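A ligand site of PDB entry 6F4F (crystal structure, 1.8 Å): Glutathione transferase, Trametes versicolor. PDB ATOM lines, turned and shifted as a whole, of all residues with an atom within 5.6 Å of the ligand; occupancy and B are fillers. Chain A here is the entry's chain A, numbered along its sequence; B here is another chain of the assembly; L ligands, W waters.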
ATOM      1  N   PHE A  14     -18.913 -26.476 -13.162  1.00  0.00           N
ATOM      2  CA  PHE A  14     -19.845 -26.404 -14.284  1.00  0.00           C
ATOM      3  C   PHE A  14     -19.566 -27.475 -15.346  1.00  0.00           C
ATOM      4  O   PHE A  14     -20.475 -27.858 -16.069  1.00  0.00           O
ATOM      5  CB  PHE A  14     -19.799 -25.025 -14.943  1.00  0.00           C
ATOM      6  CG  PHE A  14     -18.623 -24.810 -15.833  1.00  0.00           C
ATOM      7  CD1 PHE A  14     -18.664 -25.189 -17.148  1.00  0.00           C
ATOM      8  CD2 PHE A  14     -17.482 -24.233 -15.340  1.00  0.00           C
ATOM      9  CE1 PHE A  14     -17.594 -24.995 -17.965  1.00  0.00           C
ATOM     10  CE2 PHE A  14     -16.388 -24.026 -16.191  1.00  0.00           C
ATOM     11  CZ  PHE A  14     -16.461 -24.428 -17.485  1.00  0.00           C
ATOM     12  N   SER A  15     -18.305 -27.936 -15.448  1.00  0.00           N
ATOM     13  CA  SER A  15     -17.808 -28.632 -16.627  1.00  0.00           C
ATOM     14  C   SER A  15     -18.206 -30.102 -16.741  1.00  0.00           C
ATOM     15  O   SER A  15     -17.699 -30.956 -15.992  1.00  0.00           O
ATOM     16  CB  SER A  15     -16.299 -28.543 -16.667  1.00  0.00           C
ATOM     17  OG  SER A  15     -15.849 -29.326 -17.722  1.00  0.00           O
ATOM     18  N   TYR A  17     -17.188 -32.113 -19.009  1.00  0.00           N
ATOM     19  CA  TYR A  17     -15.986 -32.861 -19.414  1.00  0.00           C
ATOM     20  C   TYR A  17     -15.141 -33.220 -18.212  1.00  0.00           C
ATOM     21  O   TYR A  17     -14.593 -34.335 -18.137  1.00  0.00           O
ATOM     22  CB  TYR A  17     -15.115 -32.069 -20.381  1.00  0.00           C
ATOM     23  CG  TYR A  17     -15.662 -31.982 -21.783  1.00  0.00           C
ATOM     24  CD1 TYR A  17     -15.642 -33.081 -22.621  1.00  0.00           C
ATOM     25  CD2 TYR A  17     -16.203 -30.792 -22.277  1.00  0.00           C
ATOM     26  CE1 TYR A  17     -16.145 -33.002 -23.929  1.00  0.00           C
ATOM     27  CE2 TYR A  17     -16.723 -30.723 -23.584  1.00  0.00           C
ATOM     28  CZ  TYR A  17     -16.670 -31.817 -24.395  1.00  0.00           C
ATOM     29  OH  TYR A  17     -17.126 -31.764 -25.701  1.00  0.00           O
ATOM     30  N   ARG A  20     -16.851 -36.009 -16.055  1.00  0.00           N
ATOM     31  CA  ARG A  20     -16.566 -37.373 -16.480  1.00  0.00           C
ATOM     32  C   ARG A  20     -15.453 -37.993 -15.651  1.00  0.00           C
ATOM     33  O   ARG A  20     -15.536 -39.149 -15.191  1.00  0.00           O
ATOM     34  CB  ARG A  20     -16.088 -37.400 -17.947  1.00  0.00           C
ATOM     35  CG  ARG A  20     -17.018 -36.917 -19.004  1.00  0.00           C
ATOM     36  CD  ARG A  20     -16.323 -36.870 -20.380  1.00  0.00           C
ATOM     37  NE  ARG A  20     -17.298 -37.041 -21.450  1.00  0.00           N
ATOM     38  CZ  ARG A  20     -17.078 -36.882 -22.744  1.00  0.00           C
ATOM     39  NH1 ARG A  20     -15.883 -36.569 -23.208  1.00  0.00           N
ATOM     40  NH2 ARG A  20     -18.068 -37.098 -23.588  1.00  0.00           N
ATOM     41  N   ILE A  39     -11.187 -21.339 -15.661  1.00  0.00           N
ATOM     42  CA  ILE A  39     -10.662 -21.374 -17.002  1.00  0.00           C
ATOM     43  C   ILE A  39     -11.317 -20.359 -17.901  1.00  0.00           C
ATOM     44  O   ILE A  39     -10.724 -19.959 -18.916  1.00  0.00           O
ATOM     45  CB  ILE A  39     -10.763 -22.799 -17.592  1.00  0.00           C
ATOM     46  CG1 ILE A  39      -9.898 -22.868 -18.820  1.00  0.00           C
ATOM     47  CG2 ILE A  39     -12.185 -23.218 -17.957  1.00  0.00           C
ATOM     48  CD1 ILE A  39      -8.371 -22.804 -18.507  1.00  0.00           C
ATOM     49  N   LEU A  40     -12.496 -19.868 -17.561  1.00  0.00           N
ATOM     50  CA  LEU A  40     -13.274 -19.087 -18.516  1.00  0.00           C
ATOM     51  C   LEU A  40     -13.140 -17.589 -18.309  1.00  0.00           C
ATOM     52  O   LEU A  40     -13.509 -16.832 -19.208  1.00  0.00           O
ATOM     53  CB  LEU A  40     -14.750 -19.480 -18.419  1.00  0.00           C
ATOM     54  CG  LEU A  40     -15.112 -20.911 -18.808  1.00  0.00           C
ATOM     55  CD1 LEU A  40     -16.618 -21.029 -18.778  1.00  0.00           C
ATOM     56  CD2 LEU A  40     -14.558 -21.392 -20.180  1.00  0.00           C
ATOM     57  N   LEU A  53      -3.188 -26.757 -24.276  1.00  0.00           N
ATOM     58  CA  LEU A  53      -4.473 -26.415 -24.916  1.00  0.00           C
ATOM     59  C   LEU A  53      -5.313 -25.445 -24.086  1.00  0.00           C
ATOM     60  O   LEU A  53      -6.299 -24.894 -24.590  1.00  0.00           O
ATOM     61  CB  LEU A  53      -5.244 -27.706 -25.218  1.00  0.00           C
ATOM     62  CG  LEU A  53      -4.644 -28.731 -26.181  1.00  0.00           C
ATOM     63  CD1 LEU A  53      -5.590 -29.953 -26.279  1.00  0.00           C
ATOM     64  CD2 LEU A  53      -4.426 -28.129 -27.548  1.00  0.00           C
ATOM     65  N   LYS A  54      -4.963 -25.247 -22.815  1.00  0.00           N
ATOM     66  CA  LYS A  54      -5.663 -24.284 -21.956  1.00  0.00           C
ATOM     67  C   LYS A  54      -7.109 -24.737 -21.712  1.00  0.00           C
ATOM     68  O   LYS A  54      -8.020 -23.927 -21.636  1.00  0.00           O
ATOM     69  CB  LYS A  54      -5.618 -22.868 -22.539  1.00  0.00           C
ATOM     70  CG  LYS A  54      -4.165 -22.311 -22.600  1.00  0.00           C
ATOM     71  CD  LYS A  54      -4.087 -20.818 -22.995  1.00  0.00           C
ATOM     72  CE  LYS A  54      -4.284 -20.591 -24.458  1.00  0.00           C
ATOM     73  NZ  LYS A  54      -4.152 -19.118 -24.720  1.00  0.00           N
ATOM     74  N   LYS A  55      -7.312 -26.046 -21.606  1.00  0.00           N
ATOM     75  CA  LYS A  55      -8.628 -26.597 -21.328  1.00  0.00           C
ATOM     76  C   LYS A  55      -8.680 -27.437 -20.055  1.00  0.00           C
ATOM     77  O   LYS A  55      -7.707 -28.094 -19.677  1.00  0.00           O
ATOM     78  CB  LYS A  55      -9.086 -27.504 -22.465  1.00  0.00           C
ATOM     79  CG  LYS A  55      -9.320 -26.742 -23.727  1.00  0.00           C
ATOM     80  CD  LYS A  55      -9.612 -27.694 -24.885  1.00  0.00           C
ATOM     81  CE  LYS A  55      -9.590 -26.977 -26.179  1.00  0.00           C
ATOM     82  NZ  LYS A  55     -10.624 -25.968 -26.258  1.00  0.00           N
ATOM     83  N   ILE A  56      -9.840 -27.481 -19.437  1.00  0.00           N
ATOM     84  CA  ILE A  56     -10.107 -28.445 -18.411  1.00  0.00           C
ATOM     85  C   ILE A  56     -11.001 -29.537 -19.007  1.00  0.00           C
ATOM     86  O   ILE A  56     -11.713 -29.273 -19.980  1.00  0.00           O
ATOM     87  CB  ILE A  56     -10.742 -27.777 -17.176  1.00  0.00           C
ATOM     88  CG1 ILE A  56     -12.113 -27.194 -17.536  1.00  0.00           C
ATOM     89  CG2 ILE A  56      -9.751 -26.747 -16.579  1.00  0.00           C
ATOM     90  CD1 ILE A  56     -12.915 -26.742 -16.363  1.00  0.00           C
ATOM     91  N   PRO A  57     -10.928 -30.769 -18.479  1.00  0.00           N
ATOM     92  CA  PRO A  57     -10.012 -31.156 -17.411  1.00  0.00           C
ATOM     93  C   PRO A  57      -8.567 -31.234 -17.877  1.00  0.00           C
ATOM     94  O   PRO A  57      -8.296 -31.407 -19.061  1.00  0.00           O
ATOM     95  CB  PRO A  57     -10.507 -32.551 -17.005  1.00  0.00           C
ATOM     96  CG  PRO A  57     -11.091 -33.114 -18.282  1.00  0.00           C
ATOM     97  CD  PRO A  57     -11.720 -31.912 -18.955  1.00  0.00           C
ATOM     98  N   GLU A  80      -7.389 -34.514 -22.393  1.00  0.00           N
ATOM     99  CA  GLU A  80      -8.569 -35.090 -23.070  1.00  0.00           C
ATOM    100  C   GLU A  80      -9.293 -36.075 -22.156  1.00  0.00           C
ATOM    101  O   GLU A  80      -8.762 -37.124 -21.754  1.00  0.00           O
ATOM    102  CB  GLU A  80      -8.232 -35.696 -24.439  1.00  0.00           C
ATOM    103  CG  GLU A  80      -7.653 -34.654 -25.419  1.00  0.00           C
ATOM    104  CD  GLU A  80      -8.669 -33.587 -25.753  1.00  0.00           C
ATOM    105  OE1 GLU A  80      -9.725 -33.963 -26.321  1.00  0.00           O
ATOM    106  OE2 GLU A  80      -8.455 -32.407 -25.408  1.00  0.00           O
ATOM    107  N   SER A  81     -10.534 -35.733 -21.838  1.00  0.00           N
ATOM    108  CA  SER A  81     -11.294 -36.476 -20.839  1.00  0.00           C
ATOM    109  C   SER A  81     -11.400 -37.980 -21.140  1.00  0.00           C
ATOM    110  O   SER A  81     -11.268 -38.822 -20.245  1.00  0.00           O
ATOM    111  CB  SER A  81     -12.665 -35.835 -20.696  1.00  0.00           C
ATOM    112  OG  SER A  81     -13.496 -35.946 -21.835  1.00  0.00           O
ATOM    113  N   LEU A  82     -11.642 -38.348 -22.393  1.00  0.00           N
ATOM    114  CA  LEU A  82     -11.830 -39.776 -22.684  1.00  0.00           C
ATOM    115  C   LEU A  82     -10.512 -40.519 -22.588  1.00  0.00           C
ATOM    116  O   LEU A  82     -10.483 -41.687 -22.202  1.00  0.00           O
ATOM    117  CB  LEU A  82     -12.486 -39.965 -24.083  1.00  0.00           C
ATOM    118  CG  LEU A  82     -13.928 -39.496 -24.226  1.00  0.00           C
ATOM    119  CD1 LEU A  82     -14.499 -39.891 -25.549  1.00  0.00           C
ATOM    120  CD2 LEU A  82     -14.801 -39.959 -23.036  1.00  0.00           C
ATOM    121  N   GLU A 116     -19.866 -38.833 -28.551  1.00  0.00           N
ATOM    122  CA  GLU A 116     -18.954 -37.820 -29.050  1.00  0.00           C
ATOM    123  C   GLU A 116     -19.108 -37.382 -30.488  1.00  0.00           C
ATOM    124  O   GLU A 116     -18.796 -36.240 -30.834  1.00  0.00           O
ATOM    125  CB  GLU A 116     -17.537 -38.324 -28.880  1.00  0.00           C
ATOM    126  CG  GLU A 116     -16.574 -37.285 -28.306  1.00  0.00           C
ATOM    127  CD  GLU A 116     -16.744 -37.084 -26.803  1.00  0.00           C
ATOM    128  OE1 GLU A 116     -15.765 -36.674 -26.153  1.00  0.00           O
ATOM    129  OE2 GLU A 116     -17.856 -37.332 -26.294  1.00  0.00           O
ATOM    130  N   ARG A 124     -24.186 -28.955 -28.078  1.00  0.00           N
ATOM    131  CA  ARG A 124     -23.482 -27.698 -28.266  1.00  0.00           C
ATOM    132  C   ARG A 124     -24.302 -26.725 -29.107  1.00  0.00           C
ATOM    133  O   ARG A 124     -24.494 -25.556 -28.733  1.00  0.00           O
ATOM    134  CB  ARG A 124     -22.115 -27.942 -28.927  1.00  0.00           C
ATOM    135  CG  ARG A 124     -21.128 -28.584 -27.989  1.00  0.00           C
ATOM    136  CD  ARG A 124     -19.821 -28.961 -28.678  1.00  0.00           C
ATOM    137  NE  ARG A 124     -18.749 -29.225 -27.704  1.00  0.00           N
ATOM    138  CZ  ARG A 124     -17.452 -29.204 -28.006  1.00  0.00           C
ATOM    139  NH1 ARG A 124     -17.050 -28.928 -29.241  1.00  0.00           N
ATOM    140  NH2 ARG A 124     -16.552 -29.442 -27.059  1.00  0.00           N
ATOM    141  N   PHE A 128     -25.557 -23.560 -27.115  1.00  0.00           N
ATOM    142  CA  PHE A 128     -24.724 -22.386 -27.328  1.00  0.00           C
ATOM    143  C   PHE A 128     -25.155 -21.558 -28.544  1.00  0.00           C
ATOM    144  O   PHE A 128     -24.866 -20.365 -28.589  1.00  0.00           O
ATOM    145  CB  PHE A 128     -23.252 -22.764 -27.508  1.00  0.00           C
ATOM    146  CG  PHE A 128     -22.618 -23.396 -26.310  1.00  0.00           C
ATOM    147  CD1 PHE A 128     -22.339 -22.650 -25.182  1.00  0.00           C
ATOM    148  CD2 PHE A 128     -22.245 -24.715 -26.333  1.00  0.00           C
ATOM    149  CE1 PHE A 128     -21.756 -23.236 -24.066  1.00  0.00           C
ATOM    150  CE2 PHE A 128     -21.657 -25.296 -25.249  1.00  0.00           C
ATOM    151  CZ  PHE A 128     -21.412 -24.565 -24.096  1.00  0.00           C
ATOM    152  N   VAL A 233     -21.054 -19.227 -17.011  1.00  0.00           N
ATOM    153  CA  VAL A 233     -20.361 -19.538 -18.243  1.00  0.00           C
ATOM    154  C   VAL A 233     -20.712 -18.479 -19.275  1.00  0.00           C
ATOM    155  O   VAL A 233     -21.879 -18.408 -19.707  1.00  0.00           O
ATOM    156  CB  VAL A 233     -20.723 -20.941 -18.752  1.00  0.00           C
ATOM    157  CG1 VAL A 233     -20.061 -21.184 -20.095  1.00  0.00           C
ATOM    158  CG2 VAL A 233     -20.308 -21.974 -17.738  1.00  0.00           C
ATOM    159  N   MET A 235     -20.418 -18.126 -22.493  1.00  0.00           N
ATOM    160  CA  MET A 235     -21.061 -18.608 -23.719  1.00  0.00           C
ATOM    161  C   MET A 235     -22.454 -19.174 -23.514  1.00  0.00           C
ATOM    162  O   MET A 235     -23.144 -19.455 -24.515  1.00  0.00           O
ATOM    163  CB  MET A 235     -20.169 -19.672 -24.356  1.00  0.00           C
ATOM    164  CG  MET A 235     -19.459 -19.205 -25.592  1.00  0.00           C
ATOM    165  SD  MET A 235     -18.526 -20.572 -26.334  1.00  0.00           S
ATOM    166  CE  MET A 235     -16.889 -20.072 -25.844  1.00  0.00           C
ATOM    167  N   LEU A 236     -22.892 -19.398 -22.276  1.00  0.00           N
ATOM    168  CA  LEU A 236     -24.287 -19.762 -22.102  1.00  0.00           C
ATOM    169  C   LEU A 236     -25.186 -18.547 -22.019  1.00  0.00           C
ATOM    170  O   LEU A 236     -26.410 -18.714 -21.985  1.00  0.00           O
ATOM    171  CB  LEU A 236     -24.505 -20.654 -20.860  1.00  0.00           C
ATOM    172  CG  LEU A 236     -24.088 -22.116 -21.079  1.00  0.00           C
ATOM    173  CD1 LEU A 236     -24.203 -22.917 -19.800  1.00  0.00           C
ATOM    174  CD2 LEU A 236     -24.916 -22.789 -22.171  1.00  0.00           C
ATOM    175  N   ASN B 117     -10.964 -34.529 -32.004  1.00  0.00           N
ATOM    176  CA  ASN B 117     -11.663 -33.374 -31.482  1.00  0.00           C
ATOM    177  C   ASN B 117     -11.266 -32.051 -32.157  1.00  0.00           C
ATOM    178  O   ASN B 117     -12.122 -31.154 -32.249  1.00  0.00           O
ATOM    179  CB  ASN B 117     -11.460 -33.290 -29.965  1.00  0.00           C
ATOM    180  CG  ASN B 117     -12.254 -34.340 -29.195  1.00  0.00           C
ATOM    181  OD1 ASN B 117     -13.448 -34.501 -29.446  1.00  0.00           O
ATOM    182  ND2 ASN B 117     -11.636 -34.973 -28.209  1.00  0.00           N
ATOM    183  N   TYR B 118     -10.000 -31.871 -32.562  1.00  0.00           N
ATOM    184  CA  TYR B 118      -9.505 -30.581 -33.056  1.00  0.00           C
ATOM    185  C   TYR B 118      -9.057 -30.572 -34.526  1.00  0.00           C
ATOM    186  O   TYR B 118      -9.039 -29.489 -35.133  1.00  0.00           O
ATOM    187  CB  TYR B 118      -8.385 -30.051 -32.143  1.00  0.00           C
ATOM    188  CG  TYR B 118      -8.763 -30.134 -30.670  1.00  0.00           C
ATOM    189  CD1 TYR B 118      -9.918 -29.493 -30.213  1.00  0.00           C
ATOM    190  CD2 TYR B 118      -8.037 -30.931 -29.762  1.00  0.00           C
ATOM    191  CE1 TYR B 118     -10.335 -29.639 -28.913  1.00  0.00           C
ATOM    192  CE2 TYR B 118      -8.428 -31.058 -28.450  1.00  0.00           C
ATOM    193  CZ  TYR B 118      -9.578 -30.388 -28.029  1.00  0.00           C
ATOM    194  OH  TYR B 118     -10.011 -30.548 -26.739  1.00  0.00           O
HETATM  195  N1  LIG L   1     -12.076 -32.734 -25.823  1.00  0.00           N
HETATM  196  C1  LIG L   1     -11.845 -32.069 -24.558  1.00  0.00           C
HETATM  197  C2  LIG L   1     -12.007 -33.114 -23.421  1.00  0.00           C
HETATM  198  O1  LIG L   1     -12.683 -34.160 -23.668  1.00  0.00           O
HETATM  199  O2  LIG L   1     -11.494 -32.992 -22.267  1.00  0.00           O
HETATM  200  C3  LIG L   1     -12.807 -30.915 -24.372  1.00  0.00           C
HETATM  201  C4  LIG L   1     -12.411 -30.114 -23.136  1.00  0.00           C
HETATM  202  C5  LIG L   1     -13.116 -28.752 -23.214  1.00  0.00           C
HETATM  203  O3  LIG L   1     -13.702 -28.357 -24.165  1.00  0.00           O
HETATM  204  N2  LIG L   1     -12.948 -27.978 -22.051  1.00  0.00           N
HETATM  205  C6  LIG L   1     -13.457 -26.678 -21.743  1.00  0.00           C
HETATM  206  C7  LIG L   1     -12.460 -25.566 -21.692  1.00  0.00           C
HETATM  207  O4  LIG L   1     -11.720 -25.690 -20.767  1.00  0.00           O
HETATM  208  C8  LIG L   1     -14.786 -26.592 -21.034  1.00  0.00           C
HETATM  209  S1  LIG L   1     -15.626 -25.009 -21.278  1.00  0.00           S
HETATM  210  N3  LIG L   1     -12.364 -24.447 -22.629  1.00  0.00           N
HETATM  211  C9  LIG L   1     -11.355 -23.423 -22.415  1.00  0.00           C
HETATM  212  C10 LIG L   1     -10.666 -23.039 -23.727  1.00  0.00           C
HETATM  213  O5  LIG L   1     -10.929 -23.694 -24.775  1.00  0.00           O
HETATM  214  O6  LIG L   1      -9.835 -22.076 -23.726  1.00  0.00           O
HETATM  215  C11 LIG L   1     -16.501 -25.143 -22.823  1.00  0.00           C
HETATM  216  C12 LIG L   1     -17.227 -24.076 -23.312  1.00  0.00           C
HETATM  217  C13 LIG L   1     -17.861 -24.209 -24.516  1.00  0.00           C
HETATM  218  C14 LIG L   1     -17.773 -25.380 -25.220  1.00  0.00           C
HETATM  219  C15 LIG L   1     -17.039 -26.445 -24.754  1.00  0.00           C
HETATM  220  C16 LIG L   1     -16.400 -26.320 -23.554  1.00  0.00           C
HETATM  221  N4  LIG L   1     -17.361 -22.828 -22.561  1.00  0.00           N
HETATM  222  O7  LIG L   1     -18.065 -21.774 -23.135  1.00  0.00           O
HETATM  223  O8  LIG L   1     -16.947 -22.716 -21.462  1.00  0.00           O
HETATM  224  N5  LIG L   1     -18.464 -25.478 -26.486  1.00  0.00           N
HETATM  225  O9  LIG L   1     -18.787 -24.307 -27.167  1.00  0.00           O
HETATM  226  O10 LIG L   1     -18.739 -26.527 -26.926  1.00  0.00           O
HETATM  227  O   HOH W   1     -11.620 -36.606 -24.729  1.00  0.00           O
HETATM  228  O   HOH W   2     -19.787 -29.052 -25.057  1.00  0.00           O
HETATM  229  O   HOH W   3     -14.680 -33.975 -26.759  1.00  0.00           O
HETATM  230  O   HOH W   4     -17.830 -19.450 -22.012  1.00  0.00           O
HETATM  231  O   HOH W   5     -13.956 -24.438 -25.120  1.00  0.00           O
HETATM  232  O   HOH W   6     -13.989 -28.530 -26.723  1.00  0.00           O
HETATM  233  O   HOH W   7     -13.514 -31.060 -27.811  1.00  0.00           O
HETATM  234  O   HOH W   8      -9.009 -32.113 -21.579  1.00  0.00           O
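The guanidinium group (NE) of Arg 124 is in hydrogen-bond range of an oxygen (O10) of the ligand (2.8 Å). OE1 of Glu 80 lies within salt-bridge range of N1 of the ligand (2.7 Å). N of Ser 81 sits at hydrogen-bond distance from O2 of the ligand, 2.9 Å away. The backbone carbonyl oxygen (O) of Ile 56 lies within hydrogen-bond range of a nitrogen (N2) of the ligand. N of Ile 56 is in hydrogen-bond range of O4 of the ligand (2.9 Å). NZ of Lys 55 is in salt-bridge range of O5 of the ligand (2.7 Å). OH of Tyr 118 of chain B is in hydrogen-bond range of N1 of the ligand, at 3.1 Å. The side-chain hydroxyl of Ser 81 lies within hydrogen-bond range of an oxygen (O1) of the ligand. ND2 of Asn 117 of chain B sits close to N1 of the ligand.
The side-chain hydroxyl of Tyr 17 is in hydrogen-bond range of the guanidinium group of Arg 124 (2.8 Å). The side-chain carboxylate (OE1) of Glu 80 lies within hydrogen-bond range of the side-chain amide nitrogen (ND2) of Asn 117 of chain B, 2.9 Å away. OH of Tyr 118 of chain B sits at hydrogen-bond distance from OE2 of Glu 80. The guanidinium group (NH1) of Arg 20 is in hydrogen-bond range of the side-chain hydroxyl (OG) of Ser 81 (2.8 Å). N of Tyr 17 sits close to OG of Ser 15 (3.3 Å).
Water W6 lies within hydrogen-bond range of O3 of the ligand (2.6 Å) and NH2 of Arg 124 (2.7 Å). Water W4 lies within hydrogen-bond range of an oxygen (O7) of the ligand and the backbone NH (N) of Met 235. Water W8 lies within hydrogen-bond range of the backbone carbonyl oxygen of Pro 57 (2.7 Å), an oxygen (O2) of the ligand (2.7 Å) and the backbone NH of Glu 80 (3.0 Å). Water W1 lies within hydrogen-bond range of an oxygen (O1) of the ligand (2.9 Å), the backbone NH (N) of Leu 82 (2.9 Å) and the backbone NH (N) of Ser 81 (3.2 Å). Water W3 lies within hydrogen-bond range of the side-chain carboxylate of Glu 116 (3.0 Å), the side-chain amide oxygen of Asn 117 of chain B (3.0 Å), a nitrogen (N1) of the ligand (3.0 Å) and the side-chain hydroxyl of Tyr 17 (3.5 Å). Water W2 bridges the guanidinium group of Arg 124 and an oxygen (O10) of the ligand.
An oxygen (O6) of the ligand sits close to the backbone carbonyl oxygen (O) of Lys 54, 3.3 Å away. SD of Met 235 sits close to O7 of the ligand, 3.4 Å away. Residues that only touch the ligand: Leu 40 (3.0 Å), Tyr 17 (3.3 Å), Phe 128 (3.4 Å), Pro 57 (3.5 Å), Val 233 (3.7 Å), Ile 39 (3.8 Å) and Phe 14 (3.9 Å). Hydrophobic or aromatic side chains that line the ligand: Phe 14, Tyr 17, Ile 39, Leu 40, Ile 56, Pro 57, Phe 128, Val 233 and Met 235. Of the 22 residues printed, 16 come within 4 Å of the ligand. The nearest printed residue that does not touch the ligand is Arg 20 (4.03 Å).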
